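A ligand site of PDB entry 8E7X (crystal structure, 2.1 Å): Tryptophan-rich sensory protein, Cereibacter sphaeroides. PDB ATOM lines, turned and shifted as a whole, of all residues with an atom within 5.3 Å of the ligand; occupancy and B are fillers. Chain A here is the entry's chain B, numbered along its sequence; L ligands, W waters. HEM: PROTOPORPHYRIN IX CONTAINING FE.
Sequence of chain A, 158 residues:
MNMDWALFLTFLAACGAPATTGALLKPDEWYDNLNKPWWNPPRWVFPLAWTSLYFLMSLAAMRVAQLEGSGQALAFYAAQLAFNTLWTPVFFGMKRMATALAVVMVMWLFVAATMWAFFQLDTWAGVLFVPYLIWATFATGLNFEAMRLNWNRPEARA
Water W2 lies within hydrogen-bond range of O of Asn 84 (2.6 Å), OG1 of Thr 88 (2.8 Å), OG1 of Thr 21 (3.0 Å) and O of Thr 85 (3.4 Å).
OG1 of Thr 51 lies within hydrogen-bond range of O of Pro 47 (2.7 Å).
The side-chain amide nitrogen (ND2) of Asn 84 lies close to the side-chain sulfur (SD) of Met 107, at 3.8 Å.
The backbone carbonyl oxygen (O) of Pro 18 sits at hydrogen-bond distance from the side-chain hydroxyl (OG1) of Thr 21 (2.6 Å).
The side-chain amide oxygen (OD1) of Asn 84 sits at hydrogen-bond distance from the side-chain hydroxyl (OH) of Tyr 54.
The indole nitrogen (NE1) of Trp 87 is in hydrogen-bond range of the side-chain amide oxygen (OD1) of Asn 143.
O of Pro 27 is in hydrogen-bond range of NH2 of Arg 43, at 2.6 Å.
The side-chain amino group of Lys 26 lies within salt-bridge range of an oxygen (O2D) of the ligand (3.98 Å).
The guanidinium group (NH1) of Arg 43 is in salt-bridge range of an oxygen (O1D) of the ligand, at 2.9 Å.
NB of the ligand sits close to NE1 of Trp 50, at 3.1 Å.
Pro 18 touches the ligand (O to CMA, 3.98 Å).
C of Gly 22 touches CBA of the ligand (3.6 Å).
Ala 23 touches the ligand (CA to O2A, 3.9 Å).
CD of Pro 27 touches CBD of the ligand, 3.4 Å away.
Tyr 31 touches the ligand.
Phe 46 touches the ligand (CB to C4D, 3.4 Å).
Pro 47 touches the ligand (CB to O1A, 3.7 Å).
CE2 of Tyr 54 touches CMA of the ligand, 3.9 Å away.
Asn 84 touches the ligand.
Trp 87 touches the ligand.
Thr 88 touches the ligand (OG1 to CHB, 3.5 Å).
CZ of Phe 92 touches CHD of the ligand, at 3.4 Å.
SD of Met 107 touches CBB of the ligand, at 3.3 Å.
Ala 139 touches the ligand (O to CMC, 3.5 Å).
Leu 142 touches the ligand.
Hydrophobic or aromatic side chains that line the ligand: Pro 27, Tyr 31, Phe 46, Pro 47, Trp 50, Tyr 54, Trp 87, Phe 92, Met 107 and Leu 142.
Within 4 Å of the ligand: Pro 18, Gly 22, Ala 23, Lys 26, Pro 27, Tyr 31, Arg 43, Phe 46, Pro 47, Trp 50, Tyr 54, Asn 84, Trp 87, Thr 88, Phe 92, Met 107, Ala 139 and Leu 142.
The nearest printed residue that does not touch the ligand is Val 104 (4.1 Å).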
ATOM      1  N   PRO A  18     -24.326  21.753   9.677  1.00  0.00           N
ATOM      2  CA  PRO A  18     -23.500  22.467   8.686  1.00  0.00           C
ATOM      3  C   PRO A  18     -22.037  22.052   8.725  1.00  0.00           C
ATOM      4  O   PRO A  18     -21.393  22.015   7.673  1.00  0.00           O
ATOM      5  CB  PRO A  18     -23.670  23.942   9.064  1.00  0.00           C
ATOM      6  CG  PRO A  18     -24.067  23.929  10.493  1.00  0.00           C
ATOM      7  CD  PRO A  18     -24.916  22.702  10.650  1.00  0.00           C
ATOM      8  N   ALA A  19     -21.499  21.720   9.900  1.00  0.00           N
ATOM      9  CA  ALA A  19     -20.128  21.230   9.953  1.00  0.00           C
ATOM     10  C   ALA A  19     -19.970  19.972   9.104  1.00  0.00           C
ATOM     11  O   ALA A  19     -18.935  19.759   8.470  1.00  0.00           O
ATOM     12  CB  ALA A  19     -19.708  20.966  11.398  1.00  0.00           C
ATOM     13  N   THR A  21     -21.658  19.217   6.337  1.00  0.00           N
ATOM     14  CA  THR A  21     -21.609  19.542   4.904  1.00  0.00           C
ATOM     15  C   THR A  21     -20.191  19.886   4.478  1.00  0.00           C
ATOM     16  O   THR A  21     -19.766  19.512   3.374  1.00  0.00           O
ATOM     17  CB  THR A  21     -22.549  20.717   4.557  1.00  0.00           C
ATOM     18  OG1 THR A  21     -22.105  21.922   5.184  1.00  0.00           O
ATOM     19  CG2 THR A  21     -23.980  20.430   4.966  1.00  0.00           C
ATOM     20  N   GLY A  22     -19.440  20.575   5.333  1.00  0.00           N
ATOM     21  CA  GLY A  22     -18.072  20.907   5.006  1.00  0.00           C
ATOM     22  C   GLY A  22     -17.165  19.693   4.974  1.00  0.00           C
ATOM     23  O   GLY A  22     -16.281  19.595   4.104  1.00  0.00           O
ATOM     24  N   ALA A  23     -17.360  18.766   5.911  1.00  0.00           N
ATOM     25  CA  ALA A  23     -16.494  17.578   5.956  1.00  0.00           C
ATOM     26  C   ALA A  23     -16.742  16.646   4.774  1.00  0.00           C
ATOM     27  O   ALA A  23     -15.810  15.988   4.317  1.00  0.00           O
ATOM     28  CB  ALA A  23     -16.709  16.839   7.272  1.00  0.00           C
ATOM     29  N   LYS A  26     -15.384  18.712   0.676  1.00  0.00           N
ATOM     30  CA  LYS A  26     -14.217  19.574   0.622  1.00  0.00           C
ATOM     31  C   LYS A  26     -14.084  20.116  -0.802  1.00  0.00           C
ATOM     32  O   LYS A  26     -14.363  19.398  -1.769  1.00  0.00           O
ATOM     33  CB  LYS A  26     -12.961  18.801   1.003  1.00  0.00           C
ATOM     34  CG  LYS A  26     -12.917  18.357   2.440  1.00  0.00           C
ATOM     35  CD  LYS A  26     -11.658  18.863   3.118  1.00  0.00           C
ATOM     36  CE  LYS A  26     -10.451  18.782   2.193  1.00  0.00           C
ATOM     37  NZ  LYS A  26      -9.178  18.734   2.967  1.00  0.00           N
ATOM     38  N   PRO A  27     -13.652  21.362  -0.969  1.00  0.00           N
ATOM     39  CA  PRO A  27     -13.399  21.880  -2.321  1.00  0.00           C
ATOM     40  C   PRO A  27     -12.280  21.109  -3.002  1.00  0.00           C
ATOM     41  O   PRO A  27     -11.230  20.857  -2.404  1.00  0.00           O
ATOM     42  CB  PRO A  27     -13.033  23.342  -2.069  1.00  0.00           C
ATOM     43  CG  PRO A  27     -13.629  23.682  -0.735  1.00  0.00           C
ATOM     44  CD  PRO A  27     -13.579  22.414   0.070  1.00  0.00           C
ATOM     45  N   TYR A  31     -12.931  23.715  -7.569  1.00  0.00           N
ATOM     46  CA  TYR A  31     -12.794  24.966  -6.847  1.00  0.00           C
ATOM     47  C   TYR A  31     -11.445  25.609  -7.118  1.00  0.00           C
ATOM     48  O   TYR A  31     -11.357  26.835  -7.284  1.00  0.00           O
ATOM     49  CB  TYR A  31     -12.993  24.753  -5.348  1.00  0.00           C
ATOM     50  CG  TYR A  31     -12.622  25.957  -4.498  1.00  0.00           C
ATOM     51  CD1 TYR A  31     -13.475  27.045  -4.382  1.00  0.00           C
ATOM     52  CD2 TYR A  31     -11.407  26.007  -3.833  1.00  0.00           C
ATOM     53  CE1 TYR A  31     -13.135  28.138  -3.605  1.00  0.00           C
ATOM     54  CE2 TYR A  31     -11.054  27.101  -3.063  1.00  0.00           C
ATOM     55  CZ  TYR A  31     -11.924  28.156  -2.953  1.00  0.00           C
ATOM     56  OH  TYR A  31     -11.576  29.242  -2.193  1.00  0.00           O
ATOM     57  N   ARG A  43      -6.976  28.266   1.888  1.00  0.00           N
ATOM     58  CA  ARG A  43      -7.940  27.236   2.265  1.00  0.00           C
ATOM     59  C   ARG A  43      -8.018  27.068   3.786  1.00  0.00           C
ATOM     60  O   ARG A  43      -9.109  26.838   4.328  1.00  0.00           O
ATOM     61  CB  ARG A  43      -7.561  25.892   1.635  1.00  0.00           C
ATOM     62  CG  ARG A  43      -8.055  25.652   0.218  1.00  0.00           C
ATOM     63  CD  ARG A  43      -7.550  24.294  -0.238  1.00  0.00           C
ATOM     64  NE  ARG A  43      -8.070  23.869  -1.536  1.00  0.00           N
ATOM     65  CZ  ARG A  43      -9.056  22.986  -1.687  1.00  0.00           C
ATOM     66  NH1 ARG A  43      -9.643  22.447  -0.628  1.00  0.00           N
ATOM     67  NH2 ARG A  43      -9.454  22.647  -2.910  1.00  0.00           N
ATOM     68  N   PHE A  46     -10.761  28.903   6.181  1.00  0.00           N
ATOM     69  CA  PHE A  46     -12.190  28.586   6.292  1.00  0.00           C
ATOM     70  C   PHE A  46     -12.503  27.655   7.457  1.00  0.00           C
ATOM     71  O   PHE A  46     -13.436  27.967   8.223  1.00  0.00           O
ATOM     72  CB  PHE A  46     -12.700  28.045   4.951  1.00  0.00           C
ATOM     73  CG  PHE A  46     -12.683  29.070   3.831  1.00  0.00           C
ATOM     74  CD1 PHE A  46     -13.730  29.961   3.677  1.00  0.00           C
ATOM     75  CD2 PHE A  46     -11.606  29.136   2.955  1.00  0.00           C
ATOM     76  CE1 PHE A  46     -13.718  30.906   2.655  1.00  0.00           C
ATOM     77  CE2 PHE A  46     -11.579  30.074   1.932  1.00  0.00           C
ATOM     78  CZ  PHE A  46     -12.638  30.964   1.784  1.00  0.00           C
ATOM     79  N   PRO A  47     -11.815  26.523   7.659  1.00  0.00           N
ATOM     80  CA  PRO A  47     -12.128  25.698   8.841  1.00  0.00           C
ATOM     81  C   PRO A  47     -11.891  26.429  10.166  1.00  0.00           C
ATOM     82  O   PRO A  47     -12.654  26.199  11.122  1.00  0.00           O
ATOM     83  CB  PRO A  47     -11.204  24.484   8.689  1.00  0.00           C
ATOM     84  CG  PRO A  47     -10.195  24.873   7.659  1.00  0.00           C
ATOM     85  CD  PRO A  47     -10.866  25.848   6.765  1.00  0.00           C
ATOM     86  N   TRP A  50     -15.043  28.977  10.485  1.00  0.00           N
ATOM     87  CA  TRP A  50     -16.329  28.345  10.756  1.00  0.00           C
ATOM     88  C   TRP A  50     -16.347  27.669  12.119  1.00  0.00           C
ATOM     89  O   TRP A  50     -17.380  27.695  12.804  1.00  0.00           O
ATOM     90  CB  TRP A  50     -16.672  27.372   9.631  1.00  0.00           C
ATOM     91  CG  TRP A  50     -17.242  28.112   8.456  1.00  0.00           C
ATOM     92  CD1 TRP A  50     -16.733  28.164   7.197  1.00  0.00           C
ATOM     93  CD2 TRP A  50     -18.396  28.960   8.470  1.00  0.00           C
ATOM     94  NE1 TRP A  50     -17.522  28.969   6.401  1.00  0.00           N
ATOM     95  CE2 TRP A  50     -18.550  29.472   7.167  1.00  0.00           C
ATOM     96  CE3 TRP A  50     -19.334  29.323   9.444  1.00  0.00           C
ATOM     97  CZ2 TRP A  50     -19.591  30.328   6.810  1.00  0.00           C
ATOM     98  CZ3 TRP A  50     -20.366  30.178   9.102  1.00  0.00           C
ATOM     99  CH2 TRP A  50     -20.485  30.673   7.786  1.00  0.00           C
ATOM    100  N   THR A  51     -15.244  27.050  12.537  1.00  0.00           N
ATOM    101  CA  THR A  51     -15.223  26.428  13.861  1.00  0.00           C
ATOM    102  C   THR A  51     -15.400  27.478  14.956  1.00  0.00           C
ATOM    103  O   THR A  51     -16.173  27.273  15.899  1.00  0.00           O
ATOM    104  CB  THR A  51     -13.923  25.647  14.067  1.00  0.00           C
ATOM    105  OG1 THR A  51     -13.782  24.665  13.034  1.00  0.00           O
ATOM    106  CG2 THR A  51     -13.915  24.944  15.429  1.00  0.00           C
ATOM    107  N   TYR A  54     -19.157  28.745  14.817  1.00  0.00           N
ATOM    108  CA  TYR A  54     -20.098  27.791  15.382  1.00  0.00           C
ATOM    109  C   TYR A  54     -20.076  27.832  16.909  1.00  0.00           C
ATOM    110  O   TYR A  54     -21.119  27.752  17.562  1.00  0.00           O
ATOM    111  CB  TYR A  54     -19.821  26.384  14.838  1.00  0.00           C
ATOM    112  CG  TYR A  54     -20.175  26.251  13.369  1.00  0.00           C
ATOM    113  CD1 TYR A  54     -21.260  26.951  12.846  1.00  0.00           C
ATOM    114  CD2 TYR A  54     -19.428  25.467  12.501  1.00  0.00           C
ATOM    115  CE1 TYR A  54     -21.586  26.865  11.509  1.00  0.00           C
ATOM    116  CE2 TYR A  54     -19.757  25.369  11.145  1.00  0.00           C
ATOM    117  CZ  TYR A  54     -20.844  26.079  10.663  1.00  0.00           C
ATOM    118  OH  TYR A  54     -21.208  26.024   9.321  1.00  0.00           O
ATOM    119  N   PHE A  83     -30.302  27.862   6.483  1.00  0.00           N
ATOM    120  CA  PHE A  83     -29.698  28.315   5.234  1.00  0.00           C
ATOM    121  C   PHE A  83     -28.178  28.197   5.274  1.00  0.00           C
ATOM    122  O   PHE A  83     -27.547  28.025   4.223  1.00  0.00           O
ATOM    123  CB  PHE A  83     -30.131  29.755   4.939  1.00  0.00           C
ATOM    124  CG  PHE A  83     -31.544  29.861   4.453  1.00  0.00           C
ATOM    125  CD1 PHE A  83     -31.857  29.656   3.110  1.00  0.00           C
ATOM    126  CD2 PHE A  83     -32.575  30.136   5.330  1.00  0.00           C
ATOM    127  CE1 PHE A  83     -33.167  29.724   2.659  1.00  0.00           C
ATOM    128  CE2 PHE A  83     -33.889  30.207   4.888  1.00  0.00           C
ATOM    129  CZ  PHE A  83     -34.181  30.003   3.554  1.00  0.00           C
ATOM    130  N   ASN A  84     -27.593  28.288   6.465  1.00  0.00           N
ATOM    131  CA  ASN A  84     -26.172  27.995   6.624  1.00  0.00           C
ATOM    132  C   ASN A  84     -25.874  26.551   6.218  1.00  0.00           C
ATOM    133  O   ASN A  84     -24.904  26.280   5.498  1.00  0.00           O
ATOM    134  CB  ASN A  84     -25.753  28.259   8.069  1.00  0.00           C
ATOM    135  CG  ASN A  84     -24.262  28.061   8.313  1.00  0.00           C
ATOM    136  OD1 ASN A  84     -23.762  26.946   8.301  1.00  0.00           O
ATOM    137  ND2 ASN A  84     -23.542  29.160   8.556  1.00  0.00           N
ATOM    138  N   THR A  85     -26.715  25.614   6.657  1.00  0.00           N
ATOM    139  CA  THR A  85     -26.549  24.206   6.296  1.00  0.00           C
ATOM    140  C   THR A  85     -26.774  23.982   4.814  1.00  0.00           C
ATOM    141  O   THR A  85     -26.159  23.084   4.224  1.00  0.00           O
ATOM    142  CB  THR A  85     -27.522  23.342   7.112  1.00  0.00           C
ATOM    143  OG1 THR A  85     -27.386  23.650   8.502  1.00  0.00           O
ATOM    144  CG2 THR A  85     -27.266  21.852   6.891  1.00  0.00           C
ATOM    145  N   TRP A  87     -26.033  25.943   2.215  1.00  0.00           N
ATOM    146  CA  TRP A  87     -25.194  26.592   1.207  1.00  0.00           C
ATOM    147  C   TRP A  87     -24.165  25.654   0.588  1.00  0.00           C
ATOM    148  O   TRP A  87     -24.045  25.580  -0.636  1.00  0.00           O
ATOM    149  CB  TRP A  87     -24.505  27.818   1.814  1.00  0.00           C
ATOM    150  CG  TRP A  87     -23.797  28.571   0.756  1.00  0.00           C
ATOM    151  CD1 TRP A  87     -24.312  29.571  -0.024  1.00  0.00           C
ATOM    152  CD2 TRP A  87     -22.457  28.353   0.299  1.00  0.00           C
ATOM    153  NE1 TRP A  87     -23.359  30.005  -0.911  1.00  0.00           N
ATOM    154  CE2 TRP A  87     -22.210  29.269  -0.739  1.00  0.00           C
ATOM    155  CE3 TRP A  87     -21.426  27.483   0.680  1.00  0.00           C
ATOM    156  CZ2 TRP A  87     -20.991  29.345  -1.409  1.00  0.00           C
ATOM    157  CZ3 TRP A  87     -20.225  27.546   0.019  1.00  0.00           C
ATOM    158  CH2 TRP A  87     -20.018  28.472  -1.017  1.00  0.00           C
ATOM    159  N   THR A  88     -23.369  24.963   1.412  1.00  0.00           N
ATOM    160  CA  THR A  88     -22.285  24.137   0.853  1.00  0.00           C
ATOM    161  C   THR A  88     -22.784  23.101  -0.151  1.00  0.00           C
ATOM    162  O   THR A  88     -22.181  22.999  -1.230  1.00  0.00           O
ATOM    163  CB  THR A  88     -21.465  23.495   1.968  1.00  0.00           C
ATOM    164  OG1 THR A  88     -20.867  24.511   2.780  1.00  0.00           O
ATOM    165  CG2 THR A  88     -20.356  22.607   1.386  1.00  0.00           C
ATOM    166  N   PHE A  91     -23.503  24.998  -3.513  1.00  0.00           N
ATOM    167  CA  PHE A  91     -22.348  25.525  -4.236  1.00  0.00           C
ATOM    168  C   PHE A  91     -21.346  24.421  -4.571  1.00  0.00           C
ATOM    169  O   PHE A  91     -20.917  24.287  -5.721  1.00  0.00           O
ATOM    170  CB  PHE A  91     -21.681  26.635  -3.432  1.00  0.00           C
ATOM    171  CG  PHE A  91     -20.623  27.408  -4.211  1.00  0.00           C
ATOM    172  CD1 PHE A  91     -19.319  26.947  -4.278  1.00  0.00           C
ATOM    173  CD2 PHE A  91     -20.951  28.588  -4.856  1.00  0.00           C
ATOM    174  CE1 PHE A  91     -18.360  27.652  -4.980  1.00  0.00           C
ATOM    175  CE2 PHE A  91     -19.980  29.294  -5.565  1.00  0.00           C
ATOM    176  CZ  PHE A  91     -18.684  28.824  -5.620  1.00  0.00           C
ATOM    177  N   PHE A  92     -20.938  23.647  -3.566  1.00  0.00           N
ATOM    178  CA  PHE A  92     -19.890  22.648  -3.784  1.00  0.00           C
ATOM    179  C   PHE A  92     -20.433  21.294  -4.199  1.00  0.00           C
ATOM    180  O   PHE A  92     -19.757  20.568  -4.934  1.00  0.00           O
ATOM    181  CB  PHE A  92     -19.018  22.523  -2.527  1.00  0.00           C
ATOM    182  CG  PHE A  92     -18.040  23.646  -2.370  1.00  0.00           C
ATOM    183  CD1 PHE A  92     -17.041  23.853  -3.310  1.00  0.00           C
ATOM    184  CD2 PHE A  92     -18.139  24.529  -1.303  1.00  0.00           C
ATOM    185  CE1 PHE A  92     -16.143  24.896  -3.178  1.00  0.00           C
ATOM    186  CE2 PHE A  92     -17.245  25.576  -1.163  1.00  0.00           C
ATOM    187  CZ  PHE A  92     -16.245  25.758  -2.105  1.00  0.00           C
ATOM    188  N   VAL A 104     -26.942  32.325   0.204  1.00  0.00           N
ATOM    189  CA  VAL A 104     -26.081  33.030   1.144  1.00  0.00           C
ATOM    190  C   VAL A 104     -26.618  34.437   1.429  1.00  0.00           C
ATOM    191  O   VAL A 104     -26.384  34.986   2.512  1.00  0.00           O
ATOM    192  CB  VAL A 104     -24.622  33.044   0.657  1.00  0.00           C
ATOM    193  CG1 VAL A 104     -24.447  33.986  -0.525  1.00  0.00           C
ATOM    194  CG2 VAL A 104     -23.677  33.421   1.795  1.00  0.00           C
ATOM    195  N   MET A 107     -29.390  33.827   3.937  1.00  0.00           N
ATOM    196  CA  MET A 107     -28.706  33.575   5.200  1.00  0.00           C
ATOM    197  C   MET A 107     -28.190  34.870   5.811  1.00  0.00           C
ATOM    198  O   MET A 107     -28.349  35.099   7.015  1.00  0.00           O
ATOM    199  CB  MET A 107     -27.545  32.591   5.000  1.00  0.00           C
ATOM    200  CG  MET A 107     -26.815  32.248   6.306  1.00  0.00           C
ATOM    201  SD  MET A 107     -25.216  31.414   6.060  1.00  0.00           S
ATOM    202  CE  MET A 107     -24.094  32.813   5.985  1.00  0.00           C
ATOM    203  N   ALA A 139     -18.518  35.898   2.710  1.00  0.00           N
ATOM    204  CA  ALA A 139     -19.015  34.729   1.989  1.00  0.00           C
ATOM    205  C   ALA A 139     -19.872  35.137   0.800  1.00  0.00           C
ATOM    206  O   ALA A 139     -19.760  34.559  -0.288  1.00  0.00           O
ATOM    207  CB  ALA A 139     -19.811  33.836   2.937  1.00  0.00           C
ATOM    208  N   LEU A 142     -17.591  36.384  -1.898  1.00  0.00           N
ATOM    209  CA  LEU A 142     -16.893  35.267  -2.529  1.00  0.00           C
ATOM    210  C   LEU A 142     -17.802  34.538  -3.503  1.00  0.00           C
ATOM    211  O   LEU A 142     -17.374  34.155  -4.603  1.00  0.00           O
ATOM    212  CB  LEU A 142     -16.359  34.308  -1.468  1.00  0.00           C
ATOM    213  CG  LEU A 142     -15.057  34.696  -0.772  1.00  0.00           C
ATOM    214  CD1 LEU A 142     -14.775  33.790   0.427  1.00  0.00           C
ATOM    215  CD2 LEU A 142     -13.887  34.651  -1.761  1.00  0.00           C
ATOM    216  N   ASN A 143     -19.057  34.317  -3.114  1.00  0.00           N
ATOM    217  CA  ASN A 143     -20.020  33.683  -4.010  1.00  0.00           C
ATOM    218  C   ASN A 143     -20.266  34.551  -5.236  1.00  0.00           C
ATOM    219  O   ASN A 143     -20.347  34.036  -6.361  1.00  0.00           O
ATOM    220  CB  ASN A 143     -21.327  33.426  -3.260  1.00  0.00           C
ATOM    221  CG  ASN A 143     -22.186  32.349  -3.893  1.00  0.00           C
ATOM    222  OD1 ASN A 143     -22.859  31.595  -3.190  1.00  0.00           O
ATOM    223  ND2 ASN A 143     -22.178  32.278  -5.234  1.00  0.00           N
ATOM    224  N   ALA A 146     -17.065  34.551  -7.441  1.00  0.00           N
ATOM    225  CA  ALA A 146     -16.934  33.273  -8.132  1.00  0.00           C
ATOM    226  C   ALA A 146     -17.769  33.262  -9.402  1.00  0.00           C
ATOM    227  O   ALA A 146     -17.356  32.689 -10.422  1.00  0.00           O
ATOM    228  CB  ALA A 146     -17.356  32.140  -7.198  1.00  0.00           C
HETATM  229  CHA HEM L   1     -14.496  24.868   4.364  1.00  0.00           C
HETATM  230  CHB HEM L   1     -19.128  26.026   5.410  1.00  0.00           C
HETATM  231  CHC HEM L   1     -18.883  29.730   2.279  1.00  0.00           C
HETATM  232  CHD HEM L   1     -14.920  27.655   0.410  1.00  0.00           C
HETATM  233  C1A HEM L   1     -15.716  24.956   5.027  1.00  0.00           C
HETATM  234  C2A HEM L   1     -16.066  24.353   6.291  1.00  0.00           C
HETATM  235  C3A HEM L   1     -17.326  24.667   6.584  1.00  0.00           C
HETATM  236  C4A HEM L   1     -17.853  25.485   5.501  1.00  0.00           C
HETATM  237  CMA HEM L   1     -18.099  24.245   7.853  1.00  0.00           C
HETATM  238  CAA HEM L   1     -15.132  23.512   7.185  1.00  0.00           C
HETATM  239  CBA HEM L   1     -15.085  22.045   6.775  1.00  0.00           C
HETATM  240  CGA HEM L   1     -14.334  21.308   7.852  1.00  0.00           C
HETATM  241  O1A HEM L   1     -13.956  21.966   8.861  1.00  0.00           O
HETATM  242  O2A HEM L   1     -14.124  20.077   7.718  1.00  0.00           O
HETATM  243  C1B HEM L   1     -19.472  27.141   4.680  1.00  0.00           C
HETATM  244  C2B HEM L   1     -20.732  27.863   4.733  1.00  0.00           C
HETATM  245  C3B HEM L   1     -20.656  28.888   3.857  1.00  0.00           C
HETATM  246  C4B HEM L   1     -19.356  28.851   3.231  1.00  0.00           C
HETATM  247  CMB HEM L   1     -21.903  27.462   5.653  1.00  0.00           C
HETATM  248  CAB HEM L   1     -21.691  29.985   3.500  1.00  0.00           C
HETATM  249  CBB HEM L   1     -22.884  30.124   4.085  1.00  0.00           C
HETATM  250  C1C HEM L   1     -17.813  29.470   1.447  1.00  0.00           C
HETATM  251  C2C HEM L   1     -17.450  30.205   0.241  1.00  0.00           C
HETATM  252  C3C HEM L   1     -16.338  29.639  -0.258  1.00  0.00           C
HETATM  253  C4C HEM L   1     -15.990  28.513   0.582  1.00  0.00           C
HETATM  254  CMC HEM L   1     -18.231  31.438  -0.282  1.00  0.00           C
HETATM  255  CAC HEM L   1     -15.543  30.001  -1.541  1.00  0.00           C
HETATM  256  CBC HEM L   1     -16.116  30.547  -2.629  1.00  0.00           C
HETATM  257  C1D HEM L   1     -14.378  26.832   1.386  1.00  0.00           C
HETATM  258  C2D HEM L   1     -13.006  26.378   1.460  1.00  0.00           C
HETATM  259  C3D HEM L   1     -12.877  25.604   2.544  1.00  0.00           C
HETATM  260  C4D HEM L   1     -14.169  25.541   3.201  1.00  0.00           C
HETATM  261  CMD HEM L   1     -11.891  26.729   0.443  1.00  0.00           C
HETATM  262  CAD HEM L   1     -11.560  24.927   2.993  1.00  0.00           C
HETATM  263  CBD HEM L   1     -11.555  23.441   2.665  1.00  0.00           C
HETATM  264  CGD HEM L   1     -10.254  22.830   3.094  1.00  0.00           C
HETATM  265  O1D HEM L   1      -9.296  22.794   2.265  1.00  0.00           O
HETATM  266  O2D HEM L   1     -10.152  22.368   4.262  1.00  0.00           O
HETATM  267  NA  HEM L   1     -16.840  25.633   4.578  1.00  0.00           N
HETATM  268  NB  HEM L   1     -18.667  27.776   3.756  1.00  0.00           N
HETATM  269  NC  HEM L   1     -16.901  28.452   1.617  1.00  0.00           N
HETATM  270  ND  HEM L   1     -15.054  26.305   2.461  1.00  0.00           N
HETATM  271 FE   HEM L   1     -16.888  27.046   3.094  1.00  0.00          FE
HETATM  272  O   HOH W   1     -14.908  21.553   3.456  1.00  0.00           O
HETATM  273  O   HOH W   2     -23.163  24.629   4.408  1.00  0.00           O
HETATM  274  O   HOH W   3     -18.439  25.217   2.084  1.00  0.00           O
HETATM  275  O   HOH W   4     -16.680  31.273   4.206  1.00  0.00           O
